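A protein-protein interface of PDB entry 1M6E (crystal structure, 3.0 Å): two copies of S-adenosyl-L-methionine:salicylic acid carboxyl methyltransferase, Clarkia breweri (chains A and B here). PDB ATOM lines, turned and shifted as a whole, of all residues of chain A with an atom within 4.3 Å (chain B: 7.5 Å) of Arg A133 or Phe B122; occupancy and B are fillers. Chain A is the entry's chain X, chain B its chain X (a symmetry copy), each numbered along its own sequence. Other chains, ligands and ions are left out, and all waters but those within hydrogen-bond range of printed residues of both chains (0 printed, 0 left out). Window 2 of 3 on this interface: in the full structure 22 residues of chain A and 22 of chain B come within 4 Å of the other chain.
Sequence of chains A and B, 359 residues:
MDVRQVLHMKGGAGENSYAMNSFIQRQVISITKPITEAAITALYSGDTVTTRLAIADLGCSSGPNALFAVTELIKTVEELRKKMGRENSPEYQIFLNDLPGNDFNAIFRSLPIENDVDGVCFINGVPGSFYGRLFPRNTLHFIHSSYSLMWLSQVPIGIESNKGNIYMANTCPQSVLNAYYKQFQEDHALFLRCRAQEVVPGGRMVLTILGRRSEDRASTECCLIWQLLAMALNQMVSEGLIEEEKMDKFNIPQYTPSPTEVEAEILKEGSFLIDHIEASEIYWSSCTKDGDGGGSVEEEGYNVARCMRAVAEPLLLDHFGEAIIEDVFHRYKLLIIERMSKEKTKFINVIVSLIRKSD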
ATOM      1  N   GLY A 132       7.630  21.773 -29.864  1.00  0.00           N
ATOM      2  CA  GLY A 132       6.222  21.528 -30.070  1.00  0.00           C
ATOM      3  C   GLY A 132       5.665  21.056 -28.740  1.00  0.00           C
ATOM      4  O   GLY A 132       6.385  21.023 -27.733  1.00  0.00           O
ATOM      5  N   ARG A 133       4.396  20.669 -28.700  1.00  0.00           N
ATOM      6  CA  ARG A 133       3.864  20.250 -27.423  1.00  0.00           C
ATOM      7  C   ARG A 133       3.982  18.767 -27.156  1.00  0.00           C
ATOM      8  O   ARG A 133       3.678  17.943 -28.003  1.00  0.00           O
ATOM      9  CB  ARG A 133       2.439  20.776 -27.252  1.00  0.00           C
ATOM     10  CG  ARG A 133       2.498  22.226 -26.742  1.00  0.00           C
ATOM     11  CD  ARG A 133       1.162  22.774 -26.316  1.00  0.00           C
ATOM     12  NE  ARG A 133       0.704  22.298 -25.015  1.00  0.00           N
ATOM     13  CZ  ARG A 133      -0.446  21.658 -24.816  1.00  0.00           C
ATOM     14  NH1 ARG A 133      -1.260  21.402 -25.830  1.00  0.00           N
ATOM     15  NH2 ARG A 133      -0.798  21.296 -23.599  1.00  0.00           N
ATOM     16  N   LEU A 134       4.463  18.432 -25.965  1.00  0.00           N
ATOM     17  CA  LEU A 134       4.659  17.043 -25.592  1.00  0.00           C
ATOM     18  C   LEU A 134       3.699  16.590 -24.502  1.00  0.00           C
ATOM     19  O   LEU A 134       3.364  15.410 -24.422  1.00  0.00           O
ATOM     20  CB  LEU A 134       6.113  16.846 -25.160  1.00  0.00           C
ATOM     21  CG  LEU A 134       7.121  17.278 -26.244  1.00  0.00           C
ATOM     22  CD1 LEU A 134       8.435  17.741 -25.609  1.00  0.00           C
ATOM     23  CD2 LEU A 134       7.374  16.145 -27.207  1.00  0.00           C
ATOM     24  N   PHE A 135       3.228  17.523 -23.675  1.00  0.00           N
ATOM     25  CA  PHE A 135       2.310  17.184 -22.579  1.00  0.00           C
ATOM     26  C   PHE A 135       1.127  18.119 -22.567  1.00  0.00           C
ATOM     27  O   PHE A 135       1.213  19.251 -23.066  1.00  0.00           O
ATOM     28  CB  PHE A 135       2.999  17.310 -21.199  1.00  0.00           C
ATOM     29  CG  PHE A 135       4.414  16.810 -21.177  1.00  0.00           C
ATOM     30  CD1 PHE A 135       5.444  17.596 -21.709  1.00  0.00           C
ATOM     31  CD2 PHE A 135       4.689  15.500 -20.769  1.00  0.00           C
ATOM     32  CE1 PHE A 135       6.727  17.082 -21.858  1.00  0.00           C
ATOM     33  CE2 PHE A 135       5.949  14.980 -20.909  1.00  0.00           C
ATOM     34  CZ  PHE A 135       6.980  15.763 -21.458  1.00  0.00           C
ATOM     35  N   PRO A 136       0.007  17.665 -21.986  1.00  0.00           N
ATOM     36  CA  PRO A 136      -1.226  18.441 -21.866  1.00  0.00           C
ATOM     37  C   PRO A 136      -0.972  19.753 -21.131  1.00  0.00           C
ATOM     38  O   PRO A 136       0.115  19.960 -20.601  1.00  0.00           O
ATOM     39  CB  PRO A 136      -2.129  17.495 -21.104  1.00  0.00           C
ATOM     40  CG  PRO A 136      -1.793  16.217 -21.728  1.00  0.00           C
ATOM     41  CD  PRO A 136      -0.269  16.253 -21.713  1.00  0.00           C
ATOM     42  N   ARG A 137      -1.956  20.650 -21.112  1.00  0.00           N
ATOM     43  CA  ARG A 137      -1.770  21.948 -20.449  1.00  0.00           C
ATOM     44  C   ARG A 137      -1.655  21.801 -18.942  1.00  0.00           C
ATOM     45  O   ARG A 137      -2.278  20.917 -18.351  1.00  0.00           O
ATOM     46  CB  ARG A 137      -2.911  22.901 -20.797  1.00  0.00           C
ATOM     47  CG  ARG A 137      -2.822  23.433 -22.177  1.00  0.00           C
ATOM     48  CD  ARG A 137      -3.612  24.699 -22.330  1.00  0.00           C
ATOM     49  NE  ARG A 137      -4.178  24.747 -23.667  1.00  0.00           N
ATOM     50  CZ  ARG A 137      -5.118  23.909 -24.102  1.00  0.00           C
ATOM     51  NH1 ARG A 137      -5.601  22.965 -23.292  1.00  0.00           N
ATOM     52  NH2 ARG A 137      -5.561  24.000 -25.356  1.00  0.00           N
ATOM     53  N   CYS A 194       5.561  26.587 -25.972  1.00  0.00           N
ATOM     54  CA  CYS A 194       5.072  25.266 -25.659  1.00  0.00           C
ATOM     55  C   CYS A 194       5.281  24.960 -24.204  1.00  0.00           C
ATOM     56  O   CYS A 194       4.356  24.554 -23.497  1.00  0.00           O
ATOM     57  CB  CYS A 194       5.805  24.237 -26.504  1.00  0.00           C
ATOM     58  SG  CYS A 194       5.571  24.408 -28.278  1.00  0.00           S
ATOM     59  N   GLN A 197       2.900  26.533 -21.869  1.00  0.00           N
ATOM     60  CA  GLN A 197       1.546  26.039 -21.747  1.00  0.00           C
ATOM     61  C   GLN A 197       1.414  24.812 -20.881  1.00  0.00           C
ATOM     62  O   GLN A 197       0.332  24.526 -20.347  1.00  0.00           O
ATOM     63  CB  GLN A 197       0.992  25.664 -23.102  1.00  0.00           C
ATOM     64  CG  GLN A 197       0.800  26.759 -24.097  1.00  0.00           C
ATOM     65  CD  GLN A 197      -0.307  26.385 -25.064  1.00  0.00           C
ATOM     66  OE1 GLN A 197      -1.490  26.304 -24.671  1.00  0.00           O
ATOM     67  NE2 GLN A 197       0.061  26.123 -26.324  1.00  0.00           N
ATOM     68  N   GLU A 198       2.504  24.069 -20.756  1.00  0.00           N
ATOM     69  CA  GLU A 198       2.469  22.823 -20.000  1.00  0.00           C
ATOM     70  C   GLU A 198       3.027  22.938 -18.597  1.00  0.00           C
ATOM     71  O   GLU A 198       2.740  22.118 -17.740  1.00  0.00           O
ATOM     72  CB  GLU A 198       3.239  21.744 -20.770  1.00  0.00           C
ATOM     73  CG  GLU A 198       2.913  21.690 -22.258  1.00  0.00           C
ATOM     74  CD  GLU A 198       3.997  21.022 -23.053  1.00  0.00           C
ATOM     75  OE1 GLU A 198       5.182  21.324 -22.784  1.00  0.00           O
ATOM     76  OE2 GLU A 198       3.664  20.215 -23.942  1.00  0.00           O
ATOM     77  N   ARG B  52      -9.146  17.022 -19.922  1.00  0.00           N
ATOM     78  CA  ARG B  52      -8.164  15.948 -20.118  1.00  0.00           C
ATOM     79  C   ARG B  52      -8.731  14.555 -20.034  1.00  0.00           C
ATOM     80  O   ARG B  52      -9.335  14.184 -19.040  1.00  0.00           O
ATOM     81  CB  ARG B  52      -7.056  16.048 -19.082  1.00  0.00           C
ATOM     82  CG  ARG B  52      -5.706  15.566 -19.574  1.00  0.00           C
ATOM     83  CD  ARG B  52      -4.629  15.719 -18.498  1.00  0.00           C
ATOM     84  NE  ARG B  52      -4.485  14.501 -17.698  1.00  0.00           N
ATOM     85  CZ  ARG B  52      -5.012  14.299 -16.490  1.00  0.00           C
ATOM     86  NH1 ARG B  52      -5.741  15.240 -15.883  1.00  0.00           N
ATOM     87  NH2 ARG B  52      -4.822  13.127 -15.897  1.00  0.00           N
ATOM     88  N   ILE B  55      -6.511   7.894 -21.621  1.00  0.00           N
ATOM     89  CA  ILE B  55      -6.651   6.493 -21.951  1.00  0.00           C
ATOM     90  C   ILE B  55      -5.295   5.821 -21.793  1.00  0.00           C
ATOM     91  O   ILE B  55      -4.266   6.456 -22.028  1.00  0.00           O
ATOM     92  CB  ILE B  55      -7.100   6.363 -23.399  1.00  0.00           C
ATOM     93  CG1 ILE B  55      -8.317   7.257 -23.622  1.00  0.00           C
ATOM     94  CG2 ILE B  55      -7.398   4.911 -23.733  1.00  0.00           C
ATOM     95  CD1 ILE B  55      -8.934   7.138 -25.008  1.00  0.00           C
ATOM     96  N   ILE B  74     -10.455   7.767 -29.026  1.00  0.00           N
ATOM     97  CA  ILE B  74     -10.244   9.183 -29.258  1.00  0.00           C
ATOM     98  C   ILE B  74     -11.133   9.502 -30.444  1.00  0.00           C
ATOM     99  O   ILE B  74     -11.610  10.625 -30.601  1.00  0.00           O
ATOM    100  CB  ILE B  74      -8.768   9.470 -29.558  1.00  0.00           C
ATOM    101  CG1 ILE B  74      -7.948   9.102 -28.316  1.00  0.00           C
ATOM    102  CG2 ILE B  74      -8.580  10.942 -29.959  1.00  0.00           C
ATOM    103  CD1 ILE B  74      -6.468   9.270 -28.467  1.00  0.00           C
ATOM    104  N   GLU B  91      -7.729  17.105 -24.397  1.00  0.00           N
ATOM    105  CA  GLU B  91      -6.425  16.723 -24.941  1.00  0.00           C
ATOM    106  C   GLU B  91      -6.322  15.250 -24.570  1.00  0.00           C
ATOM    107  O   GLU B  91      -6.675  14.865 -23.448  1.00  0.00           O
ATOM    108  CB  GLU B  91      -5.294  17.494 -24.270  1.00  0.00           C
ATOM    109  CG  GLU B  91      -5.143  18.897 -24.779  1.00  0.00           C
ATOM    110  CD  GLU B  91      -4.084  19.686 -24.030  1.00  0.00           C
ATOM    111  OE1 GLU B  91      -4.220  19.833 -22.791  1.00  0.00           O
ATOM    112  OE2 GLU B  91      -3.126  20.166 -24.683  1.00  0.00           O
ATOM    113  N   TYR B  92      -5.871  14.408 -25.490  1.00  0.00           N
ATOM    114  CA  TYR B  92      -5.787  13.003 -25.140  1.00  0.00           C
ATOM    115  C   TYR B  92      -4.408  12.668 -24.641  1.00  0.00           C
ATOM    116  O   TYR B  92      -3.408  13.058 -25.260  1.00  0.00           O
ATOM    117  CB  TYR B  92      -6.145  12.136 -26.332  1.00  0.00           C
ATOM    118  CG  TYR B  92      -7.516  12.431 -26.841  1.00  0.00           C
ATOM    119  CD1 TYR B  92      -7.759  13.542 -27.658  1.00  0.00           C
ATOM    120  CD2 TYR B  92      -8.595  11.634 -26.460  1.00  0.00           C
ATOM    121  CE1 TYR B  92      -9.053  13.853 -28.085  1.00  0.00           C
ATOM    122  CE2 TYR B  92      -9.889  11.932 -26.878  1.00  0.00           C
ATOM    123  CZ  TYR B  92     -10.112  13.039 -27.688  1.00  0.00           C
ATOM    124  OH  TYR B  92     -11.400  13.309 -28.080  1.00  0.00           O
ATOM    125  N   GLN B  93      -4.347  11.989 -23.497  1.00  0.00           N
ATOM    126  CA  GLN B  93      -3.057  11.603 -22.951  1.00  0.00           C
ATOM    127  C   GLN B  93      -2.964  10.107 -22.831  1.00  0.00           C
ATOM    128  O   GLN B  93      -3.519   9.501 -21.919  1.00  0.00           O
ATOM    129  CB  GLN B  93      -2.821  12.223 -21.611  1.00  0.00           C
ATOM    130  CG  GLN B  93      -1.480  11.888 -21.087  1.00  0.00           C
ATOM    131  CD  GLN B  93      -1.193  12.719 -19.897  1.00  0.00           C
ATOM    132  OE1 GLN B  93      -2.055  12.848 -19.023  1.00  0.00           O
ATOM    133  NE2 GLN B  93       0.011  13.306 -19.835  1.00  0.00           N
ATOM    134  N   ILE B  94      -2.219   9.531 -23.764  1.00  0.00           N
ATOM    135  CA  ILE B  94      -2.057   8.102 -23.878  1.00  0.00           C
ATOM    136  C   ILE B  94      -0.874   7.440 -23.192  1.00  0.00           C
ATOM    137  O   ILE B  94       0.252   7.936 -23.201  1.00  0.00           O
ATOM    138  CB  ILE B  94      -2.023   7.742 -25.332  1.00  0.00           C
ATOM    139  CG1 ILE B  94      -3.249   8.328 -26.006  1.00  0.00           C
ATOM    140  CG2 ILE B  94      -1.946   6.243 -25.489  1.00  0.00           C
ATOM    141  CD1 ILE B  94      -3.311   7.966 -27.465  1.00  0.00           C
ATOM    142  N   PHE B  95      -1.158   6.285 -22.613  1.00  0.00           N
ATOM    143  CA  PHE B  95      -0.154   5.507 -21.920  1.00  0.00           C
ATOM    144  C   PHE B  95      -0.087   4.087 -22.448  1.00  0.00           C
ATOM    145  O   PHE B  95      -1.012   3.309 -22.198  1.00  0.00           O
ATOM    146  CB  PHE B  95      -0.480   5.498 -20.433  1.00  0.00           C
ATOM    147  CG  PHE B  95      -0.229   6.808 -19.770  1.00  0.00           C
ATOM    148  CD1 PHE B  95      -1.270   7.661 -19.470  1.00  0.00           C
ATOM    149  CD2 PHE B  95       1.076   7.230 -19.531  1.00  0.00           C
ATOM    150  CE1 PHE B  95      -1.011   8.929 -18.943  1.00  0.00           C
ATOM    151  CE2 PHE B  95       1.344   8.480 -19.012  1.00  0.00           C
ATOM    152  CZ  PHE B  95       0.303   9.333 -18.720  1.00  0.00           C
ATOM    153  N   ASP B 116       2.155  13.860 -34.668  1.00  0.00           N
ATOM    154  CA  ASP B 116       1.335  14.071 -33.470  1.00  0.00           C
ATOM    155  C   ASP B 116       0.104  13.179 -33.634  1.00  0.00           C
ATOM    156  O   ASP B 116       0.230  11.986 -33.918  1.00  0.00           O
ATOM    157  CB  ASP B 116       0.895  15.540 -33.353  1.00  0.00           C
ATOM    158  CG  ASP B 116       2.016  16.459 -32.882  1.00  0.00           C
ATOM    159  OD1 ASP B 116       2.559  16.230 -31.778  1.00  0.00           O
ATOM    160  OD2 ASP B 116       2.350  17.418 -33.612  1.00  0.00           O
ATOM    161  N   VAL B 117      -1.084  13.745 -33.435  1.00  0.00           N
ATOM    162  CA  VAL B 117      -2.331  12.992 -33.602  1.00  0.00           C
ATOM    163  C   VAL B 117      -3.549  13.936 -33.494  1.00  0.00           C
ATOM    164  O   VAL B 117      -3.446  15.020 -32.911  1.00  0.00           O
ATOM    165  CB  VAL B 117      -2.446  11.802 -32.574  1.00  0.00           C
ATOM    166  CG1 VAL B 117      -2.631  10.482 -33.323  1.00  0.00           C
ATOM    167  CG2 VAL B 117      -1.204  11.710 -31.689  1.00  0.00           C
ATOM    168  N   GLY B 119      -6.643  15.854 -32.356  1.00  0.00           N
ATOM    169  CA  GLY B 119      -7.196  16.265 -31.079  1.00  0.00           C
ATOM    170  C   GLY B 119      -5.987  16.456 -30.180  1.00  0.00           C
ATOM    171  O   GLY B 119      -6.098  16.812 -29.003  1.00  0.00           O
ATOM    172  N   VAL B 120      -4.822  16.235 -30.788  1.00  0.00           N
ATOM    173  CA  VAL B 120      -3.513  16.302 -30.148  1.00  0.00           C
ATOM    174  C   VAL B 120      -3.448  15.146 -29.144  1.00  0.00           C
ATOM    175  O   VAL B 120      -4.177  15.110 -28.144  1.00  0.00           O
ATOM    176  CB  VAL B 120      -3.243  17.699 -29.470  1.00  0.00           C
ATOM    177  CG1 VAL B 120      -3.665  17.698 -28.004  1.00  0.00           C
ATOM    178  CG2 VAL B 120      -1.756  18.080 -29.620  1.00  0.00           C
ATOM    179  N   CYS B 121      -2.602  14.169 -29.452  1.00  0.00           N
ATOM    180  CA  CYS B 121      -2.451  13.016 -28.587  1.00  0.00           C
ATOM    181  C   CYS B 121      -1.032  12.839 -28.098  1.00  0.00           C
ATOM    182  O   CYS B 121      -0.133  12.415 -28.816  1.00  0.00           O
ATOM    183  CB  CYS B 121      -2.892  11.749 -29.301  1.00  0.00           C
ATOM    184  SG  CYS B 121      -4.349  11.996 -30.287  1.00  0.00           S
ATOM    185  N   PHE B 122      -0.833  13.167 -26.847  1.00  0.00           N
ATOM    186  CA  PHE B 122       0.466  13.007 -26.284  1.00  0.00           C
ATOM    187  C   PHE B 122       0.699  11.534 -25.901  1.00  0.00           C
ATOM    188  O   PHE B 122       0.115  11.027 -24.937  1.00  0.00           O
ATOM    189  CB  PHE B 122       0.532  13.959 -25.115  1.00  0.00           C
ATOM    190  CG  PHE B 122       0.158  15.351 -25.500  1.00  0.00           C
ATOM    191  CD1 PHE B 122      -0.964  15.950 -24.998  1.00  0.00           C
ATOM    192  CD2 PHE B 122       0.959  16.071 -26.362  1.00  0.00           C
ATOM    193  CE1 PHE B 122      -1.272  17.242 -25.342  1.00  0.00           C
ATOM    194  CE2 PHE B 122       0.662  17.358 -26.712  1.00  0.00           C
ATOM    195  CZ  PHE B 122      -0.456  17.944 -26.195  1.00  0.00           C
ATOM    196  N   ILE B 123       1.540  10.842 -26.670  1.00  0.00           N
ATOM    197  CA  ILE B 123       1.797   9.441 -26.364  1.00  0.00           C
ATOM    198  C   ILE B 123       2.953   9.216 -25.419  1.00  0.00           C
ATOM    199  O   ILE B 123       3.990   9.864 -25.524  1.00  0.00           O
ATOM    200  CB  ILE B 123       2.037   8.609 -27.618  1.00  0.00           C
ATOM    201  CG1 ILE B 123       0.730   8.510 -28.402  1.00  0.00           C
ATOM    202  CG2 ILE B 123       2.535   7.216 -27.226  1.00  0.00           C
ATOM    203  CD1 ILE B 123       0.831   7.774 -29.680  1.00  0.00           C
ATOM    204  N   ASN B 124       2.750   8.286 -24.493  1.00  0.00           N
ATOM    205  CA  ASN B 124       3.739   7.953 -23.489  1.00  0.00           C
ATOM    206  C   ASN B 124       3.841   6.445 -23.327  1.00  0.00           C
ATOM    207  O   ASN B 124       2.816   5.773 -23.171  1.00  0.00           O
ATOM    208  CB  ASN B 124       3.353   8.562 -22.130  1.00  0.00           C
ATOM    209  CG  ASN B 124       3.117  10.066 -22.195  1.00  0.00           C
ATOM    210  OD1 ASN B 124       4.005  10.832 -22.554  1.00  0.00           O
ATOM    211  ND2 ASN B 124       1.913  10.492 -21.839  1.00  0.00           N
ATOM    212  N   GLY B 125       5.069   5.922 -23.369  1.00  0.00           N
ATOM    213  CA  GLY B 125       5.316   4.497 -23.142  1.00  0.00           C
ATOM    214  C   GLY B 125       5.634   4.296 -21.649  1.00  0.00           C
ATOM    215  O   GLY B 125       6.467   4.991 -21.117  1.00  0.00           O
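No position is printed for both chains. Of the 8 pairs that touch across the chains among the printed residues, none has its exchanged pair printed and touching as well.
Of the 17 printed residues of chain B, 3 touch a printed residue of chain A. Hydrophobic or aromatic side chains of chain A that line the printed part of chain B: Pro A136. Along chain A the printed residues that touch a printed residue of chain B span positions 133 to 137.
Arg A133 touches Phe B122 (O to CE2, 3.3 Å). Leu A134 touches Phe B122 (O to CD2, 3.2 Å). C of Phe A135 touches CE1 of Phe B122, at 3.8 Å. Pro A136 touches Glu B91 (CA to OE1, 3.4 Å). Pro A136 touches Gln B93. CD1 of Phe B122 touches CD of Pro A136 (3.4 Å).
Gly A132 touches none of the printed residues of chain B. Arg A133 touches two residues of chain B. Printed residues of chain B within 4 Å of Leu A134: Phe B122. Of the printed residues of chain B, Pro A136 touches Glu B91 (3.4 Å), Gln B93 (3.5 Å) and Phe B122 (3.4 Å). Printed residues of chain A within 4 Å of Glu B91: Arg A133, Pro A136 and Arg A137. Phe B122 touches four residues of chain A. The nearest printed residue of chain A that does not touch Gln B93 is Phe A135 (5.2 Å).
The side-chain carboxylate (OE1) of Glu B91 is in salt-bridge range of the guanidinium group (NH1) of Arg A137, 3.5 Å away. The guanidinium group (NH1) of Arg A133 is in salt-bridge range of the side-chain carboxylate (OE2) of Glu B91 (2.5 Å).
OE1 of Gln A197 sits at hydrogen-bond distance from NE of Arg A137 (3.3 Å). The backbone NH of Leu A134 is in hydrogen-bond range of the side-chain carboxylate of Glu A198 (2.8 Å). The backbone carbonyl oxygen of Tyr B92 is in hydrogen-bond range of the backbone NH of Phe B122, 3.0 Å away. The backbone carbonyl oxygen (O) of Pro A136 lies close to the guanidinium group (NH2) of Arg A133 (3.4 Å). The side-chain carboxylate (OE2) of Glu A198 is in salt-bridge range of the guanidinium group (NE) of Arg A133 (3.8 Å). The backbone NH (N) of Ile B94 sits at hydrogen-bond distance from the backbone carbonyl oxygen (O) of Phe B122 (3.0 Å).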
